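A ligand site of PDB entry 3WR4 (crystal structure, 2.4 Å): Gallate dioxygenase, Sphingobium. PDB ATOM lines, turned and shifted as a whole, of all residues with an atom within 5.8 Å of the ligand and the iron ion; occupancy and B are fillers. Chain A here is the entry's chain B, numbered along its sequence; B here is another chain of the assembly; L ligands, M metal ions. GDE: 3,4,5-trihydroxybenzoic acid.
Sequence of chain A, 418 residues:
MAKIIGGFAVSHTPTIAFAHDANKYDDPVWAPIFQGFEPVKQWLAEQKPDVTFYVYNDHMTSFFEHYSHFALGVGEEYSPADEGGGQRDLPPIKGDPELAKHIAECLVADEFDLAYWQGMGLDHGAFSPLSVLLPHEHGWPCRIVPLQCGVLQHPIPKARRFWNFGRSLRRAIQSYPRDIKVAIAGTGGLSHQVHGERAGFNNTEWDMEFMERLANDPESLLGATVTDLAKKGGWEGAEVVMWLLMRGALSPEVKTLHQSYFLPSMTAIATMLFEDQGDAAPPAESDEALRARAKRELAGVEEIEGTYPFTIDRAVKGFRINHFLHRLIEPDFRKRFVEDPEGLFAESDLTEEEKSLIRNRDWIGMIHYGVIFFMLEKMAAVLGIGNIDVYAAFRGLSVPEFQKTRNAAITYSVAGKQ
OH of Tyr 391 of chain B lies within hydrogen-bond range of OAA of the ligand, at 2.7 Å. NE2 of His 59 sits close to OAE of the ligand (3.3 Å). An oxygen (OAE) of the ligand is in hydrogen-bond range of a ring nitrogen (NE2) of His 124 (3.2 Å). OH of Tyr 412 of chain B lies within hydrogen-bond range of OAA of the ligand. An oxygen (OAC) of the ligand is in hydrogen-bond range of the side-chain carboxylate of Glu 377 of chain B (2.6 Å). The side-chain hydroxyl (OG1) of Thr 267 lies within hydrogen-bond range of an oxygen (OAB) of the ligand (2.5 Å).
O of Tyr 412 of chain B is in hydrogen-bond range of N of Asn 387 of chain B (3.4 Å). The side-chain carboxylate of Glu 239 lies within hydrogen-bond range of the backbone NH of Gly 189, 3.2 Å away. The backbone NH (N) of Gly 188 is in hydrogen-bond range of a ring nitrogen (ND1) of His 12, 3.3 Å away. N of Asn 57 lies within hydrogen-bond range of SD of Met 242 (3.6 Å). OE2 of Glu 377 of chain B sits at hydrogen-bond distance from ND2 of Asn 387 of chain B. ND1 of His 12 lies within hydrogen-bond range of O of Gly 125 (3.3 Å). ND1 of His 59 sits at hydrogen-bond distance from NE2 of His 124. ND2 of Asn 387 of chain B lies within hydrogen-bond range of OH of Tyr 391 of chain B, 2.8 Å away.
Merely in contact with the ligand: Thr 13 (2.9 Å), Pro 14 (3.3 Å), His 192 (3.6 Å), Met 266 (3.7 Å), Asn 387 of chain B (3.8 Å), Phe 374 of chain B (3.8 Å) and Thr 15 (3.9 Å). 14 residues have an atom within 4 Å of the ligand: Thr 13, Pro 14, Thr 15, His 59, His 124, His 192, Glu 239, Met 266, Thr 267, Phe 374 of chain B, Glu 377 of chain B, Asn 387 of chain B, Tyr 391 of chain B and Tyr 412 of chain B. Along chain A the residues within 4 Å of the ligand span positions 13 to 267. The nearest printed residue that does not touch the ligand is Val 194 (4.1 Å).
Of the 25 residues printed, 4 come within 4 Å of the iron ion. Along chain A the residues within 4 Å of the iron ion span positions 12 to 239.
The iron ion is bound by NE2 of His 59, OE1 of Glu 239, ND2 of Asn 57 and NE2 of His 12.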
ATOM      1  N   HIS A  12      11.968   1.598 -30.901  1.00  0.00           N
ATOM      2  CA  HIS A  12      11.622   0.186 -30.712  1.00  0.00           C
ATOM      3  C   HIS A  12      10.185  -0.150 -31.099  1.00  0.00           C
ATOM      4  O   HIS A  12       9.599  -1.115 -30.588  1.00  0.00           O
ATOM      5  CB  HIS A  12      11.950  -0.293 -29.259  1.00  0.00           C
ATOM      6  CG  HIS A  12      11.355   0.508 -28.146  1.00  0.00           C
ATOM      7  ND1 HIS A  12      11.967   0.625 -26.917  1.00  0.00           N
ATOM      8  CD2 HIS A  12      10.183   1.194 -28.044  1.00  0.00           C
ATOM      9  CE1 HIS A  12      11.226   1.363 -26.110  1.00  0.00           C
ATOM     10  NE2 HIS A  12      10.142   1.731 -26.774  1.00  0.00           N
ATOM     11  N   THR A  13       9.648   0.623 -32.058  1.00  0.00           N
ATOM     12  CA  THR A  13       8.386   0.325 -32.754  1.00  0.00           C
ATOM     13  C   THR A  13       8.257  -1.127 -33.147  1.00  0.00           C
ATOM     14  O   THR A  13       9.142  -1.626 -33.791  1.00  0.00           O
ATOM     15  CB  THR A  13       8.253   1.069 -34.074  1.00  0.00           C
ATOM     16  OG1 THR A  13       8.846   2.361 -34.002  1.00  0.00           O
ATOM     17  CG2 THR A  13       6.816   1.145 -34.463  1.00  0.00           C
ATOM     18  N   PRO A  14       7.121  -1.784 -32.837  1.00  0.00           N
ATOM     19  CA  PRO A  14       6.903  -3.153 -33.317  1.00  0.00           C
ATOM     20  C   PRO A  14       6.888  -3.228 -34.840  1.00  0.00           C
ATOM     21  O   PRO A  14       7.120  -4.321 -35.357  1.00  0.00           O
ATOM     22  CB  PRO A  14       5.536  -3.513 -32.750  1.00  0.00           C
ATOM     23  CG  PRO A  14       4.845  -2.184 -32.589  1.00  0.00           C
ATOM     24  CD  PRO A  14       5.956  -1.289 -32.085  1.00  0.00           C
ATOM     25  N   THR A  15       6.652  -2.117 -35.530  1.00  0.00           N
ATOM     26  CA  THR A  15       6.714  -2.107 -36.998  1.00  0.00           C
ATOM     27  C   THR A  15       8.068  -2.580 -37.511  1.00  0.00           C
ATOM     28  O   THR A  15       8.158  -3.181 -38.581  1.00  0.00           O
ATOM     29  CB  THR A  15       6.472  -0.702 -37.605  1.00  0.00           C
ATOM     30  OG1 THR A  15       7.535   0.187 -37.218  1.00  0.00           O
ATOM     31  CG2 THR A  15       5.137  -0.137 -37.171  1.00  0.00           C
ATOM     32  N   ASN A  57      11.620   0.089 -22.628  1.00  0.00           N
ATOM     33  CA  ASN A  57      10.491  -0.132 -21.726  1.00  0.00           C
ATOM     34  C   ASN A  57       9.616  -1.242 -22.255  1.00  0.00           C
ATOM     35  O   ASN A  57       9.457  -1.411 -23.464  1.00  0.00           O
ATOM     36  CB  ASN A  57       9.641   1.126 -21.488  1.00  0.00           C
ATOM     37  CG  ASN A  57       8.712   1.460 -22.669  1.00  0.00           C
ATOM     38  OD1 ASN A  57       7.542   1.060 -22.742  1.00  0.00           O
ATOM     39  ND2 ASN A  57       9.251   2.207 -23.609  1.00  0.00           N
ATOM     40  N   HIS A  59       5.826  -2.885 -22.548  1.00  0.00           N
ATOM     41  CA  HIS A  59       4.576  -2.206 -22.896  1.00  0.00           C
ATOM     42  C   HIS A  59       3.359  -2.941 -22.319  1.00  0.00           C
ATOM     43  O   HIS A  59       2.552  -3.545 -23.050  1.00  0.00           O
ATOM     44  CB  HIS A  59       4.510  -2.068 -24.425  1.00  0.00           C
ATOM     45  CG  HIS A  59       5.657  -1.284 -24.996  1.00  0.00           C
ATOM     46  ND1 HIS A  59       6.852  -1.865 -25.375  1.00  0.00           N
ATOM     47  CD2 HIS A  59       5.806   0.043 -25.232  1.00  0.00           C
ATOM     48  CE1 HIS A  59       7.673  -0.934 -25.826  1.00  0.00           C
ATOM     49  NE2 HIS A  59       7.063   0.237 -25.750  1.00  0.00           N
ATOM     50  N   HIS A 124       8.265  -6.240 -27.606  1.00  0.00           N
ATOM     51  CA  HIS A 124       8.821  -5.544 -28.755  1.00  0.00           C
ATOM     52  C   HIS A 124       9.808  -4.457 -28.307  1.00  0.00           C
ATOM     53  O   HIS A 124      10.758  -4.152 -29.029  1.00  0.00           O
ATOM     54  CB  HIS A 124       7.700  -4.980 -29.650  1.00  0.00           C
ATOM     55  CG  HIS A 124       6.916  -3.839 -29.056  1.00  0.00           C
ATOM     56  ND1 HIS A 124       5.634  -3.993 -28.560  1.00  0.00           N
ATOM     57  CD2 HIS A 124       7.207  -2.523 -28.936  1.00  0.00           C
ATOM     58  CE1 HIS A 124       5.186  -2.833 -28.144  1.00  0.00           C
ATOM     59  NE2 HIS A 124       6.115  -1.918 -28.353  1.00  0.00           N
ATOM     60  N   GLY A 125       9.626  -3.928 -27.109  1.00  0.00           N
ATOM     61  CA  GLY A 125      10.588  -3.004 -26.524  1.00  0.00           C
ATOM     62  C   GLY A 125      12.041  -3.415 -26.722  1.00  0.00           C
ATOM     63  O   GLY A 125      12.899  -2.572 -27.006  1.00  0.00           O
ATOM     64  N   VAL A 151       8.122   3.902 -17.735  1.00  0.00           N
ATOM     65  CA  VAL A 151       7.830   5.217 -18.253  1.00  0.00           C
ATOM     66  C   VAL A 151       6.355   5.454 -18.660  1.00  0.00           C
ATOM     67  O   VAL A 151       5.989   6.539 -19.122  1.00  0.00           O
ATOM     68  CB  VAL A 151       8.733   5.475 -19.455  1.00  0.00           C
ATOM     69  CG1 VAL A 151      10.140   5.269 -19.019  1.00  0.00           C
ATOM     70  CG2 VAL A 151       8.360   4.535 -20.611  1.00  0.00           C
ATOM     71  N   LEU A 152       5.518   4.444 -18.478  1.00  0.00           N
ATOM     72  CA  LEU A 152       4.124   4.520 -18.865  1.00  0.00           C
ATOM     73  C   LEU A 152       3.141   4.969 -17.762  1.00  0.00           C
ATOM     74  O   LEU A 152       2.070   5.462 -18.070  1.00  0.00           O
ATOM     75  CB  LEU A 152       3.693   3.165 -19.397  1.00  0.00           C
ATOM     76  CG  LEU A 152       4.505   2.772 -20.628  1.00  0.00           C
ATOM     77  CD1 LEU A 152       4.225   1.339 -21.035  1.00  0.00           C
ATOM     78  CD2 LEU A 152       4.200   3.722 -21.811  1.00  0.00           C
ATOM     79  N   GLY A 188      13.503   3.327 -28.001  1.00  0.00           N
ATOM     80  CA  GLY A 188      12.247   4.062 -27.896  1.00  0.00           C
ATOM     81  C   GLY A 188      12.290   5.312 -28.761  1.00  0.00           C
ATOM     82  O   GLY A 188      13.282   5.571 -29.445  1.00  0.00           O
ATOM     83  N   GLY A 189      11.207   6.077 -28.725  1.00  0.00           N
ATOM     84  CA  GLY A 189      11.124   7.284 -29.527  1.00  0.00           C
ATOM     85  C   GLY A 189      11.087   6.964 -31.019  1.00  0.00           C
ATOM     86  O   GLY A 189      10.856   5.797 -31.399  1.00  0.00           O
ATOM     87  N   HIS A 192       6.036  10.480 -31.539  1.00  0.00           N
ATOM     88  CA  HIS A 192       4.888   9.628 -31.839  1.00  0.00           C
ATOM     89  C   HIS A 192       3.933   9.723 -30.659  1.00  0.00           C
ATOM     90  O   HIS A 192       4.381   9.978 -29.523  1.00  0.00           O
ATOM     91  CB  HIS A 192       5.246   8.153 -32.080  1.00  0.00           C
ATOM     92  CG  HIS A 192       5.693   7.422 -30.859  1.00  0.00           C
ATOM     93  ND1 HIS A 192       6.910   7.639 -30.251  1.00  0.00           N
ATOM     94  CD2 HIS A 192       5.081   6.460 -30.125  1.00  0.00           C
ATOM     95  CE1 HIS A 192       7.033   6.851 -29.200  1.00  0.00           C
ATOM     96  NE2 HIS A 192       5.939   6.121 -29.111  1.00  0.00           N
ATOM     97  N   VAL A 194       0.453   7.272 -29.574  1.00  0.00           N
ATOM     98  CA  VAL A 194      -0.352   6.160 -30.062  1.00  0.00           C
ATOM     99  C   VAL A 194      -1.684   5.957 -29.303  1.00  0.00           C
ATOM    100  O   VAL A 194      -2.231   4.840 -29.277  1.00  0.00           O
ATOM    101  CB  VAL A 194       0.488   4.868 -30.027  1.00  0.00           C
ATOM    102  CG1 VAL A 194       1.507   4.861 -31.188  1.00  0.00           C
ATOM    103  CG2 VAL A 194       1.181   4.723 -28.662  1.00  0.00           C
ATOM    104  N   GLU A 239       8.981   8.945 -23.836  1.00  0.00           N
ATOM    105  CA  GLU A 239       9.817   7.820 -23.444  1.00  0.00           C
ATOM    106  C   GLU A 239      11.281   8.012 -23.860  1.00  0.00           C
ATOM    107  O   GLU A 239      12.152   7.246 -23.434  1.00  0.00           O
ATOM    108  CB  GLU A 239       9.277   6.488 -24.009  1.00  0.00           C
ATOM    109  CG  GLU A 239       9.589   6.214 -25.491  1.00  0.00           C
ATOM    110  CD  GLU A 239       8.955   4.908 -26.013  1.00  0.00           C
ATOM    111  OE1 GLU A 239       8.675   4.022 -25.193  1.00  0.00           O
ATOM    112  OE2 GLU A 239       8.704   4.772 -27.242  1.00  0.00           O
ATOM    113  N   MET A 242      14.760   7.637 -21.839  1.00  0.00           N
ATOM    114  CA  MET A 242      15.661   6.503 -21.856  1.00  0.00           C
ATOM    115  C   MET A 242      16.857   6.784 -22.746  1.00  0.00           C
ATOM    116  O   MET A 242      17.933   6.246 -22.526  1.00  0.00           O
ATOM    117  CB  MET A 242      14.940   5.239 -22.314  1.00  0.00           C
ATOM    118  CG  MET A 242      14.006   4.697 -21.226  1.00  0.00           C
ATOM    119  SD  MET A 242      13.097   3.252 -21.771  1.00  0.00           S
ATOM    120  CE  MET A 242      11.864   3.987 -22.842  1.00  0.00           C
ATOM    121  N   SER A 265       4.935   5.887 -40.742  1.00  0.00           N
ATOM    122  CA  SER A 265       3.623   5.665 -40.153  1.00  0.00           C
ATOM    123  C   SER A 265       3.429   6.494 -38.876  1.00  0.00           C
ATOM    124  O   SER A 265       3.493   7.719 -38.926  1.00  0.00           O
ATOM    125  CB  SER A 265       3.435   4.178 -39.890  1.00  0.00           C
ATOM    126  OG  SER A 265       2.075   3.856 -39.692  1.00  0.00           O
ATOM    127  N   MET A 266       3.210   5.829 -37.727  1.00  0.00           N
ATOM    128  CA  MET A 266       2.995   6.528 -36.462  1.00  0.00           C
ATOM    129  C   MET A 266       4.294   7.042 -35.873  1.00  0.00           C
ATOM    130  O   MET A 266       4.312   8.074 -35.215  1.00  0.00           O
ATOM    131  CB  MET A 266       2.321   5.618 -35.439  1.00  0.00           C
ATOM    132  CG  MET A 266       1.048   5.003 -35.978  1.00  0.00           C
ATOM    133  SD  MET A 266      -0.189   6.273 -36.323  1.00  0.00           S
ATOM    134  CE  MET A 266      -0.740   6.700 -34.665  1.00  0.00           C
ATOM    135  N   THR A 267       5.371   6.303 -36.123  1.00  0.00           N
ATOM    136  CA  THR A 267       6.577   6.521 -35.372  1.00  0.00           C
ATOM    137  C   THR A 267       7.728   7.080 -36.189  1.00  0.00           C
ATOM    138  O   THR A 267       8.136   6.503 -37.192  1.00  0.00           O
ATOM    139  CB  THR A 267       7.048   5.187 -34.727  1.00  0.00           C
ATOM    140  OG1 THR A 267       5.946   4.587 -34.027  1.00  0.00           O
ATOM    141  CG2 THR A 267       8.220   5.414 -33.756  1.00  0.00           C
ATOM    142  N   PHE B 373      -3.352   2.119 -23.909  1.00  0.00           N
ATOM    143  CA  PHE B 373      -3.317   1.671 -25.273  1.00  0.00           C
ATOM    144  C   PHE B 373      -2.772   0.237 -25.475  1.00  0.00           C
ATOM    145  O   PHE B 373      -3.310  -0.537 -26.278  1.00  0.00           O
ATOM    146  CB  PHE B 373      -2.488   2.629 -26.122  1.00  0.00           C
ATOM    147  CG  PHE B 373      -2.185   2.094 -27.462  1.00  0.00           C
ATOM    148  CD1 PHE B 373      -3.219   1.847 -28.349  1.00  0.00           C
ATOM    149  CD2 PHE B 373      -0.889   1.804 -27.844  1.00  0.00           C
ATOM    150  CE1 PHE B 373      -2.975   1.323 -29.583  1.00  0.00           C
ATOM    151  CE2 PHE B 373      -0.630   1.279 -29.083  1.00  0.00           C
ATOM    152  CZ  PHE B 373      -1.673   1.041 -29.963  1.00  0.00           C
ATOM    153  N   PHE B 374      -1.709  -0.119 -24.766  1.00  0.00           N
ATOM    154  CA  PHE B 374      -0.996  -1.346 -25.099  1.00  0.00           C
ATOM    155  C   PHE B 374      -1.836  -2.592 -24.798  1.00  0.00           C
ATOM    156  O   PHE B 374      -1.614  -3.633 -25.417  1.00  0.00           O
ATOM    157  CB  PHE B 374       0.361  -1.344 -24.385  1.00  0.00           C
ATOM    158  CG  PHE B 374       1.118  -0.085 -24.628  1.00  0.00           C
ATOM    159  CD1 PHE B 374       1.833   0.083 -25.801  1.00  0.00           C
ATOM    160  CD2 PHE B 374       1.033   0.964 -23.740  1.00  0.00           C
ATOM    161  CE1 PHE B 374       2.502   1.275 -26.061  1.00  0.00           C
ATOM    162  CE2 PHE B 374       1.697   2.159 -23.982  1.00  0.00           C
ATOM    163  CZ  PHE B 374       2.416   2.321 -25.142  1.00  0.00           C
ATOM    164  N   GLU B 377      -3.687  -2.772 -28.081  1.00  0.00           N
ATOM    165  CA  GLU B 377      -2.743  -3.197 -29.103  1.00  0.00           C
ATOM    166  C   GLU B 377      -2.765  -4.715 -29.187  1.00  0.00           C
ATOM    167  O   GLU B 377      -2.689  -5.301 -30.263  1.00  0.00           O
ATOM    168  CB  GLU B 377      -1.343  -2.677 -28.789  1.00  0.00           C
ATOM    169  CG  GLU B 377      -0.271  -3.030 -29.803  1.00  0.00           C
ATOM    170  CD  GLU B 377       1.075  -2.395 -29.475  1.00  0.00           C
ATOM    171  OE1 GLU B 377       1.654  -2.677 -28.389  1.00  0.00           O
ATOM    172  OE2 GLU B 377       1.555  -1.585 -30.292  1.00  0.00           O
ATOM    173  N   ASN B 387      -3.004  -2.447 -35.429  1.00  0.00           N
ATOM    174  CA  ASN B 387      -2.825  -1.116 -34.914  1.00  0.00           C
ATOM    175  C   ASN B 387      -3.508   0.024 -35.693  1.00  0.00           C
ATOM    176  O   ASN B 387      -4.117   0.919 -35.086  1.00  0.00           O
ATOM    177  CB  ASN B 387      -1.331  -0.831 -34.799  1.00  0.00           C
ATOM    178  CG  ASN B 387      -0.681  -1.575 -33.644  1.00  0.00           C
ATOM    179  OD1 ASN B 387      -0.895  -2.775 -33.482  1.00  0.00           O
ATOM    180  ND2 ASN B 387       0.091  -0.869 -32.829  1.00  0.00           N
ATOM    181  N   TYR B 391      -5.855   3.131 -34.462  1.00  0.00           N
ATOM    182  CA  TYR B 391      -5.555   4.543 -34.643  1.00  0.00           C
ATOM    183  C   TYR B 391      -6.707   5.236 -35.393  1.00  0.00           C
ATOM    184  O   TYR B 391      -7.251   6.239 -34.904  1.00  0.00           O
ATOM    185  CB  TYR B 391      -4.231   4.721 -35.370  1.00  0.00           C
ATOM    186  CG  TYR B 391      -3.105   4.012 -34.709  1.00  0.00           C
ATOM    187  CD1 TYR B 391      -2.948   4.058 -33.320  1.00  0.00           C
ATOM    188  CD2 TYR B 391      -2.192   3.268 -35.445  1.00  0.00           C
ATOM    189  CE1 TYR B 391      -1.904   3.392 -32.709  1.00  0.00           C
ATOM    190  CE2 TYR B 391      -1.149   2.588 -34.832  1.00  0.00           C
ATOM    191  CZ  TYR B 391      -1.000   2.646 -33.467  1.00  0.00           C
ATOM    192  OH  TYR B 391       0.032   1.979 -32.869  1.00  0.00           O
ATOM    193  N   TYR B 412       0.408  -3.652 -39.561  1.00  0.00           N
ATOM    194  CA  TYR B 412       1.181  -4.490 -38.621  1.00  0.00           C
ATOM    195  C   TYR B 412       0.416  -4.875 -37.346  1.00  0.00           C
ATOM    196  O   TYR B 412      -0.627  -4.287 -37.039  1.00  0.00           O
ATOM    197  CB  TYR B 412       2.473  -3.776 -38.213  1.00  0.00           C
ATOM    198  CG  TYR B 412       2.250  -2.357 -37.718  1.00  0.00           C
ATOM    199  CD1 TYR B 412       2.091  -2.082 -36.360  1.00  0.00           C
ATOM    200  CD2 TYR B 412       2.191  -1.282 -38.614  1.00  0.00           C
ATOM    201  CE1 TYR B 412       1.883  -0.781 -35.901  1.00  0.00           C
ATOM    202  CE2 TYR B 412       1.979   0.025 -38.167  1.00  0.00           C
ATOM    203  CZ  TYR B 412       1.830   0.264 -36.813  1.00  0.00           C
ATOM    204  OH  TYR B 412       1.631   1.543 -36.359  1.00  0.00           O
HETATM  205  OAA GDE L   1       2.418   1.832 -34.031  1.00  0.00           O
HETATM  206  OAB GDE L   1       4.349   2.699 -34.606  1.00  0.00           O
HETATM  207  OAC GDE L   1       3.463  -0.126 -29.431  1.00  0.00           O
HETATM  208  OAD GDE L   1       7.001   2.942 -30.337  1.00  0.00           O
HETATM  209  OAE GDE L   1       5.889   1.231 -28.620  1.00  0.00           O
HETATM  210  CAF GDE L   1       3.528   0.992 -31.499  1.00  0.00           C
HETATM  211  CAG GDE L   1       5.294   2.528 -31.942  1.00  0.00           C
HETATM  212  CAH GDE L   1       3.588   2.170 -33.742  1.00  0.00           C
HETATM  213  CAI GDE L   1       4.094   0.763 -30.246  1.00  0.00           C
HETATM  214  CAJ GDE L   1       5.872   2.290 -30.705  1.00  0.00           C
HETATM  215  CAK GDE L   1       4.135   1.884 -32.362  1.00  0.00           C
HETATM  216  CAL GDE L   1       5.278   1.413 -29.840  1.00  0.00           C
HETATM  217 FE    FE M   1       8.075   2.055 -25.645  1.00  0.00          FE
